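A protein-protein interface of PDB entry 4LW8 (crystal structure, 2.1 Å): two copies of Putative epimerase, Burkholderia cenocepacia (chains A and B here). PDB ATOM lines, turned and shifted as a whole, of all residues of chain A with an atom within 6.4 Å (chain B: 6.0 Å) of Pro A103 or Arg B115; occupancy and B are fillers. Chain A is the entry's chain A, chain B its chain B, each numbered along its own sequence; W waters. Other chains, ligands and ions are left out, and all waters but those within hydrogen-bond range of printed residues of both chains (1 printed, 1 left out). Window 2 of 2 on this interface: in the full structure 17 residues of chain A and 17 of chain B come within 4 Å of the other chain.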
ATOM      1  N   GLU A 102      14.372  -6.371  -6.924  1.00  0.00           N
ATOM      2  CA  GLU A 102      13.315  -6.393  -7.927  1.00  0.00           C
ATOM      3  C   GLU A 102      12.201  -5.423  -7.562  1.00  0.00           C
ATOM      4  O   GLU A 102      11.650  -5.492  -6.457  1.00  0.00           O
ATOM      5  CB  GLU A 102      12.746  -7.806  -8.086  1.00  0.00           C
ATOM      6  N   PRO A 103      11.868  -4.512  -8.494  1.00  0.00           N
ATOM      7  CA  PRO A 103      10.805  -3.527  -8.278  1.00  0.00           C
ATOM      8  C   PRO A 103       9.493  -4.231  -7.939  1.00  0.00           C
ATOM      9  O   PRO A 103       8.749  -3.768  -7.074  1.00  0.00           O
ATOM     10  CB  PRO A 103      10.702  -2.791  -9.625  1.00  0.00           C
ATOM     11  CG  PRO A 103      11.987  -3.087 -10.336  1.00  0.00           C
ATOM     12  CD  PRO A 103      12.454  -4.428  -9.845  1.00  0.00           C
ATOM     13  N   SER A 104       9.245  -5.361  -8.597  1.00  0.00           N
ATOM     14  CA  SER A 104       8.000  -6.091  -8.415  1.00  0.00           C
ATOM     15  C   SER A 104       7.757  -6.533  -6.965  1.00  0.00           C
ATOM     16  O   SER A 104       6.615  -6.527  -6.499  1.00  0.00           O
ATOM     17  CB  SER A 104       7.972  -7.307  -9.336  1.00  0.00           C
ATOM     18  OG  SER A 104       8.862  -8.288  -8.862  1.00  0.00           O
ATOM     19  N   GLN A 105       8.812  -6.928  -6.258  1.00  0.00           N
ATOM     20  CA  GLN A 105       8.673  -7.345  -4.871  1.00  0.00           C
ATOM     21  C   GLN A 105       8.439  -6.162  -3.932  1.00  0.00           C
ATOM     22  O   GLN A 105       7.694  -6.263  -2.945  1.00  0.00           O
ATOM     23  CB  GLN A 105       9.905  -8.140  -4.426  1.00  0.00           C
ATOM     24  CG  GLN A 105       9.773  -9.631  -4.702  1.00  0.00           C
ATOM     25  CD  GLN A 105       8.561 -10.246  -3.991  1.00  0.00           C
ATOM     26  OE1 GLN A 105       7.480 -10.385  -4.581  1.00  0.00           O
ATOM     27  NE2 GLN A 105       8.740 -10.618  -2.717  1.00  0.00           N
ATOM     28  N   THR A 106       9.063  -5.041  -4.268  1.00  0.00           N
ATOM     29  CA  THR A 106       8.889  -3.794  -3.549  1.00  0.00           C
ATOM     30  C   THR A 106       7.437  -3.333  -3.605  1.00  0.00           C
ATOM     31  O   THR A 106       6.850  -2.999  -2.574  1.00  0.00           O
ATOM     32  CB  THR A 106       9.793  -2.689  -4.129  1.00  0.00           C
ATOM     33  OG1 THR A 106      11.162  -3.046  -3.912  1.00  0.00           O
ATOM     34  CG2 THR A 106       9.507  -1.347  -3.459  1.00  0.00           C
ATOM     35  N   TYR A 107       6.849  -3.333  -4.800  1.00  0.00           N
ATOM     36  CA  TYR A 107       5.432  -2.971  -4.914  1.00  0.00           C
ATOM     37  C   TYR A 107       4.513  -4.004  -4.238  1.00  0.00           C
ATOM     38  O   TYR A 107       3.605  -3.635  -3.490  1.00  0.00           O
ATOM     39  CB  TYR A 107       5.048  -2.776  -6.386  1.00  0.00           C
ATOM     40  CG  TYR A 107       5.631  -1.503  -6.964  1.00  0.00           C
ATOM     41  CD1 TYR A 107       5.175  -0.253  -6.538  1.00  0.00           C
ATOM     42  CD2 TYR A 107       6.645  -1.543  -7.918  1.00  0.00           C
ATOM     43  CE1 TYR A 107       5.693   0.931  -7.072  1.00  0.00           C
ATOM     44  CE2 TYR A 107       7.181  -0.366  -8.455  1.00  0.00           C
ATOM     45  CZ  TYR A 107       6.693   0.862  -8.027  1.00  0.00           C
ATOM     46  OH  TYR A 107       7.210   2.012  -8.548  1.00  0.00           O
ATOM     47  N   ALA A 108       4.775  -5.290  -4.463  1.00  0.00           N
ATOM     48  CA  ALA A 108       3.971  -6.352  -3.851  1.00  0.00           C
ATOM     49  C   ALA A 108       4.000  -6.293  -2.313  1.00  0.00           C
ATOM     50  O   ALA A 108       2.945  -6.197  -1.671  1.00  0.00           O
ATOM     51  CB  ALA A 108       4.444  -7.730  -4.335  1.00  0.00           C
ATOM     52  N   ASP A 159      11.160   3.757  -7.029  1.00  0.00           N
ATOM     53  CA  ASP A 159      10.056   2.801  -6.899  1.00  0.00           C
ATOM     54  C   ASP A 159       9.685   2.555  -5.450  1.00  0.00           C
ATOM     55  O   ASP A 159       8.511   2.401  -5.122  1.00  0.00           O
ATOM     56  CB  ASP A 159      10.397   1.470  -7.581  1.00  0.00           C
ATOM     57  CG  ASP A 159      10.423   1.590  -9.088  1.00  0.00           C
ATOM     58  OD1 ASP A 159       9.379   1.918  -9.694  1.00  0.00           O
ATOM     59  OD2 ASP A 159      11.482   1.386  -9.683  1.00  0.00           O
ATOM     60  N   ASN B 110      -0.836  -3.235 -13.596  1.00  0.00           N
ATOM     61  CA  ASN B 110      -0.903  -1.810 -13.861  1.00  0.00           C
ATOM     62  C   ASN B 110       0.354  -1.066 -13.465  1.00  0.00           C
ATOM     63  O   ASN B 110       0.728  -0.100 -14.132  1.00  0.00           O
ATOM     64  CB  ASN B 110      -2.146  -1.211 -13.185  1.00  0.00           C
ATOM     65  CG  ASN B 110      -3.426  -1.784 -13.776  1.00  0.00           C
ATOM     66  OD1 ASN B 110      -3.419  -2.261 -14.901  1.00  0.00           O
ATOM     67  ND2 ASN B 110      -4.506  -1.758 -13.027  1.00  0.00           N
ATOM     68  N   ILE B 111       1.048  -1.526 -12.431  1.00  0.00           N
ATOM     69  CA  ILE B 111       2.286  -0.834 -12.071  1.00  0.00           C
ATOM     70  C   ILE B 111       3.519  -1.449 -12.731  1.00  0.00           C
ATOM     71  O   ILE B 111       4.221  -0.776 -13.491  1.00  0.00           O
ATOM     72  CB  ILE B 111       2.510  -0.816 -10.561  1.00  0.00           C
ATOM     73  CG1 ILE B 111       1.331  -0.132  -9.845  1.00  0.00           C
ATOM     74  CG2 ILE B 111       3.819  -0.123 -10.244  1.00  0.00           C
ATOM     75  CD1 ILE B 111       1.412  -0.265  -8.305  1.00  0.00           C
ATOM     76  N   VAL B 112       3.777  -2.725 -12.450  1.00  0.00           N
ATOM     77  CA  VAL B 112       4.996  -3.368 -12.925  1.00  0.00           C
ATOM     78  C   VAL B 112       4.902  -3.593 -14.444  1.00  0.00           C
ATOM     79  O   VAL B 112       5.892  -3.455 -15.147  1.00  0.00           O
ATOM     80  CB  VAL B 112       5.262  -4.711 -12.202  1.00  0.00           C
ATOM     81  CG1 VAL B 112       6.518  -5.419 -12.783  1.00  0.00           C
ATOM     82  CG2 VAL B 112       5.433  -4.480 -10.704  1.00  0.00           C
ATOM     83  N   GLY B 113       3.704  -3.917 -14.937  1.00  0.00           N
ATOM     84  CA  GLY B 113       3.486  -4.107 -16.364  1.00  0.00           C
ATOM     85  C   GLY B 113       3.834  -2.843 -17.127  1.00  0.00           C
ATOM     86  O   GLY B 113       4.511  -2.886 -18.162  1.00  0.00           O
ATOM     87  N   THR B 114       3.385  -1.710 -16.598  1.00  0.00           N
ATOM     88  CA  THR B 114       3.708  -0.425 -17.192  1.00  0.00           C
ATOM     89  C   THR B 114       5.202  -0.146 -17.104  1.00  0.00           C
ATOM     90  O   THR B 114       5.812   0.296 -18.072  1.00  0.00           O
ATOM     91  CB  THR B 114       2.926   0.716 -16.513  1.00  0.00           C
ATOM     92  OG1 THR B 114       1.518   0.468 -16.649  1.00  0.00           O
ATOM     93  CG2 THR B 114       3.265   2.046 -17.147  1.00  0.00           C
ATOM     94  N   ARG B 115       5.797  -0.435 -15.950  1.00  0.00           N
ATOM     95  CA  ARG B 115       7.228  -0.237 -15.770  1.00  0.00           C
ATOM     96  C   ARG B 115       8.037  -1.066 -16.773  1.00  0.00           C
ATOM     97  O   ARG B 115       9.043  -0.588 -17.307  1.00  0.00           O
ATOM     98  CB  ARG B 115       7.661  -0.622 -14.339  1.00  0.00           C
ATOM     99  CG  ARG B 115       9.075  -0.156 -13.992  1.00  0.00           C
ATOM    100  CD  ARG B 115       9.600  -0.761 -12.664  1.00  0.00           C
ATOM    101  NE  ARG B 115      10.908  -0.193 -12.317  1.00  0.00           N
ATOM    102  CZ  ARG B 115      12.055  -0.616 -12.837  1.00  0.00           C
ATOM    103  NH1 ARG B 115      12.052  -1.612 -13.716  1.00  0.00           N
ATOM    104  NH2 ARG B 115      13.200  -0.044 -12.484  1.00  0.00           N
ATOM    105  N   ASN B 116       7.618  -2.313 -17.002  1.00  0.00           N
ATOM    106  CA  ASN B 116       8.284  -3.170 -17.991  1.00  0.00           C
ATOM    107  C   ASN B 116       8.229  -2.567 -19.384  1.00  0.00           C
ATOM    108  O   ASN B 116       9.196  -2.631 -20.138  1.00  0.00           O
ATOM    109  CB  ASN B 116       7.658  -4.566 -18.033  1.00  0.00           C
ATOM    110  CG  ASN B 116       7.934  -5.367 -16.779  1.00  0.00           C
ATOM    111  OD1 ASN B 116       8.837  -5.047 -16.011  1.00  0.00           O
ATOM    112  ND2 ASN B 116       7.163  -6.428 -16.579  1.00  0.00           N
ATOM    113  N   LEU B 117       7.088  -1.988 -19.734  1.00  0.00           N
ATOM    114  CA  LEU B 117       6.982  -1.292 -21.015  1.00  0.00           C
ATOM    115  C   LEU B 117       7.985  -0.132 -21.107  1.00  0.00           C
ATOM    116  O   LEU B 117       8.721   0.001 -22.087  1.00  0.00           O
ATOM    117  CB  LEU B 117       5.555  -0.758 -21.220  1.00  0.00           C
ATOM    118  CG  LEU B 117       5.403   0.196 -22.403  1.00  0.00           C
ATOM    119  CD1 LEU B 117       5.703  -0.545 -23.702  1.00  0.00           C
ATOM    120  CD2 LEU B 117       3.989   0.817 -22.446  1.00  0.00           C
ATOM    121  N   LEU B 118       8.010   0.703 -20.074  1.00  0.00           N
ATOM    122  CA  LEU B 118       8.875   1.872 -20.062  1.00  0.00           C
ATOM    123  C   LEU B 118      10.354   1.460 -20.084  1.00  0.00           C
ATOM    124  O   LEU B 118      11.154   2.071 -20.784  1.00  0.00           O
ATOM    125  CB  LEU B 118       8.550   2.762 -18.830  1.00  0.00           C
ATOM    126  CG  LEU B 118       7.113   3.309 -18.789  1.00  0.00           C
ATOM    127  CD1 LEU B 118       6.845   4.133 -17.537  1.00  0.00           C
ATOM    128  CD2 LEU B 118       6.785   4.104 -20.042  1.00  0.00           C
ATOM    129  N   ALA B 119      10.724   0.428 -19.325  1.00  0.00           N
ATOM    130  CA  ALA B 119      12.108  -0.042 -19.347  1.00  0.00           C
ATOM    131  C   ALA B 119      12.487  -0.529 -20.743  1.00  0.00           C
ATOM    132  O   ALA B 119      13.602  -0.278 -21.230  1.00  0.00           O
ATOM    133  CB  ALA B 119      12.333  -1.183 -18.304  1.00  0.00           C
ATOM    134  N   ALA B 120      11.556  -1.230 -21.384  1.00  0.00           N
ATOM    135  CA  ALA B 120      11.783  -1.724 -22.743  1.00  0.00           C
ATOM    136  C   ALA B 120      12.029  -0.576 -23.739  1.00  0.00           C
ATOM    137  O   ALA B 120      12.946  -0.633 -24.552  1.00  0.00           O
ATOM    138  CB  ALA B 120      10.598  -2.555 -23.185  1.00  0.00           C
ATOM    139  N   ALA B 170       4.877   5.847 -10.872  1.00  0.00           N
ATOM    140  CA  ALA B 170       5.955   4.950 -11.281  1.00  0.00           C
ATOM    141  C   ALA B 170       6.463   5.351 -12.676  1.00  0.00           C
ATOM    142  O   ALA B 170       7.652   5.265 -12.955  1.00  0.00           O
ATOM    143  CB  ALA B 170       5.490   3.495 -11.268  1.00  0.00           C
ATOM    144  N   TRP B 174      10.588   7.733 -15.133  1.00  0.00           N
ATOM    145  CA  TRP B 174      11.239   7.530 -16.422  1.00  0.00           C
ATOM    146  C   TRP B 174      11.268   8.809 -17.263  1.00  0.00           C
ATOM    147  O   TRP B 174      11.655   8.778 -18.439  1.00  0.00           O
ATOM    148  CB  TRP B 174      10.530   6.403 -17.183  1.00  0.00           C
ATOM    149  CG  TRP B 174      10.660   5.089 -16.482  1.00  0.00           C
ATOM    150  CD1 TRP B 174       9.862   4.605 -15.468  1.00  0.00           C
ATOM    151  CD2 TRP B 174      11.679   4.095 -16.699  1.00  0.00           C
ATOM    152  NE1 TRP B 174      10.318   3.367 -15.066  1.00  0.00           N
ATOM    153  CE2 TRP B 174      11.431   3.034 -15.805  1.00  0.00           C
ATOM    154  CE3 TRP B 174      12.774   4.001 -17.564  1.00  0.00           C
ATOM    155  CZ2 TRP B 174      12.235   1.890 -15.756  1.00  0.00           C
ATOM    156  CZ3 TRP B 174      13.576   2.860 -17.513  1.00  0.00           C
ATOM    157  CH2 TRP B 174      13.302   1.826 -16.612  1.00  0.00           C
HETATM  158  O   HOH W   1       9.027   2.831 -12.421  1.00  0.00           O
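The guanidinium group (NE) of Arg B115 is in salt-bridge range of the side-chain carboxylate (OD2) of Asp A159, at 3.1 Å.
The side-chain hydroxyl (OH) of Tyr A107 lies within hydrogen-bond range of the side-chain carboxylate (OD1) of Asp A159, 2.5 Å away. OD1 of Asn B116 sits close to O of Val B112.
Arg B115 touches Pro A103 (CZ to CG, 3.5 Å). CG2 of Val B112 touches CA of Ser A104, 3.8 Å away. CG2 of Ile B111 touches CZ of Tyr A107 (3.8 Å). Tyr A107 touches Ala B170 (OH to CB, 3.5 Å).
Pro A103 touches just one residue of chain B: Arg B115 (3.5 Å). Of the printed residues of chain B, Ser A104 touches Val B112. Gln A105 touches none of the printed residues of chain B. Of the printed residues of chain B, Asp A159 touches Arg B115 (3.1 Å). Printed residues of chain A within 4 Å of Ile B111: Tyr A107. Of the printed residues of chain A, Val B112 touches Ser A104. Arg B115 touches just these residues of chain A: Pro A103 and Asp A159. The nearest residue of chain A that does not touch Arg B115 is Tyr A107 (4.9 Å). The nearest printed residue of chain B that does not touch Tyr A107 is Val B112 (4.2 Å).
Of the 13 printed residues of chain B, 4 touch a printed residue of chain A. Hydrophobic or aromatic side chains of chain B that line the printed part of chain A: Ile B111, Val B112 and Ala B170. Among the printed residues, 5 pairs touch across the chains.
No position is printed for both chains. Of the 5 pairs that touch across the chains among the printed residues, none has its exchanged pair printed and touching as well.
Water W1 lies within hydrogen-bond range of the backbone carbonyl oxygen of Ala B170, the side-chain carboxylate of Asp A159 and the indole nitrogen of Trp B174.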
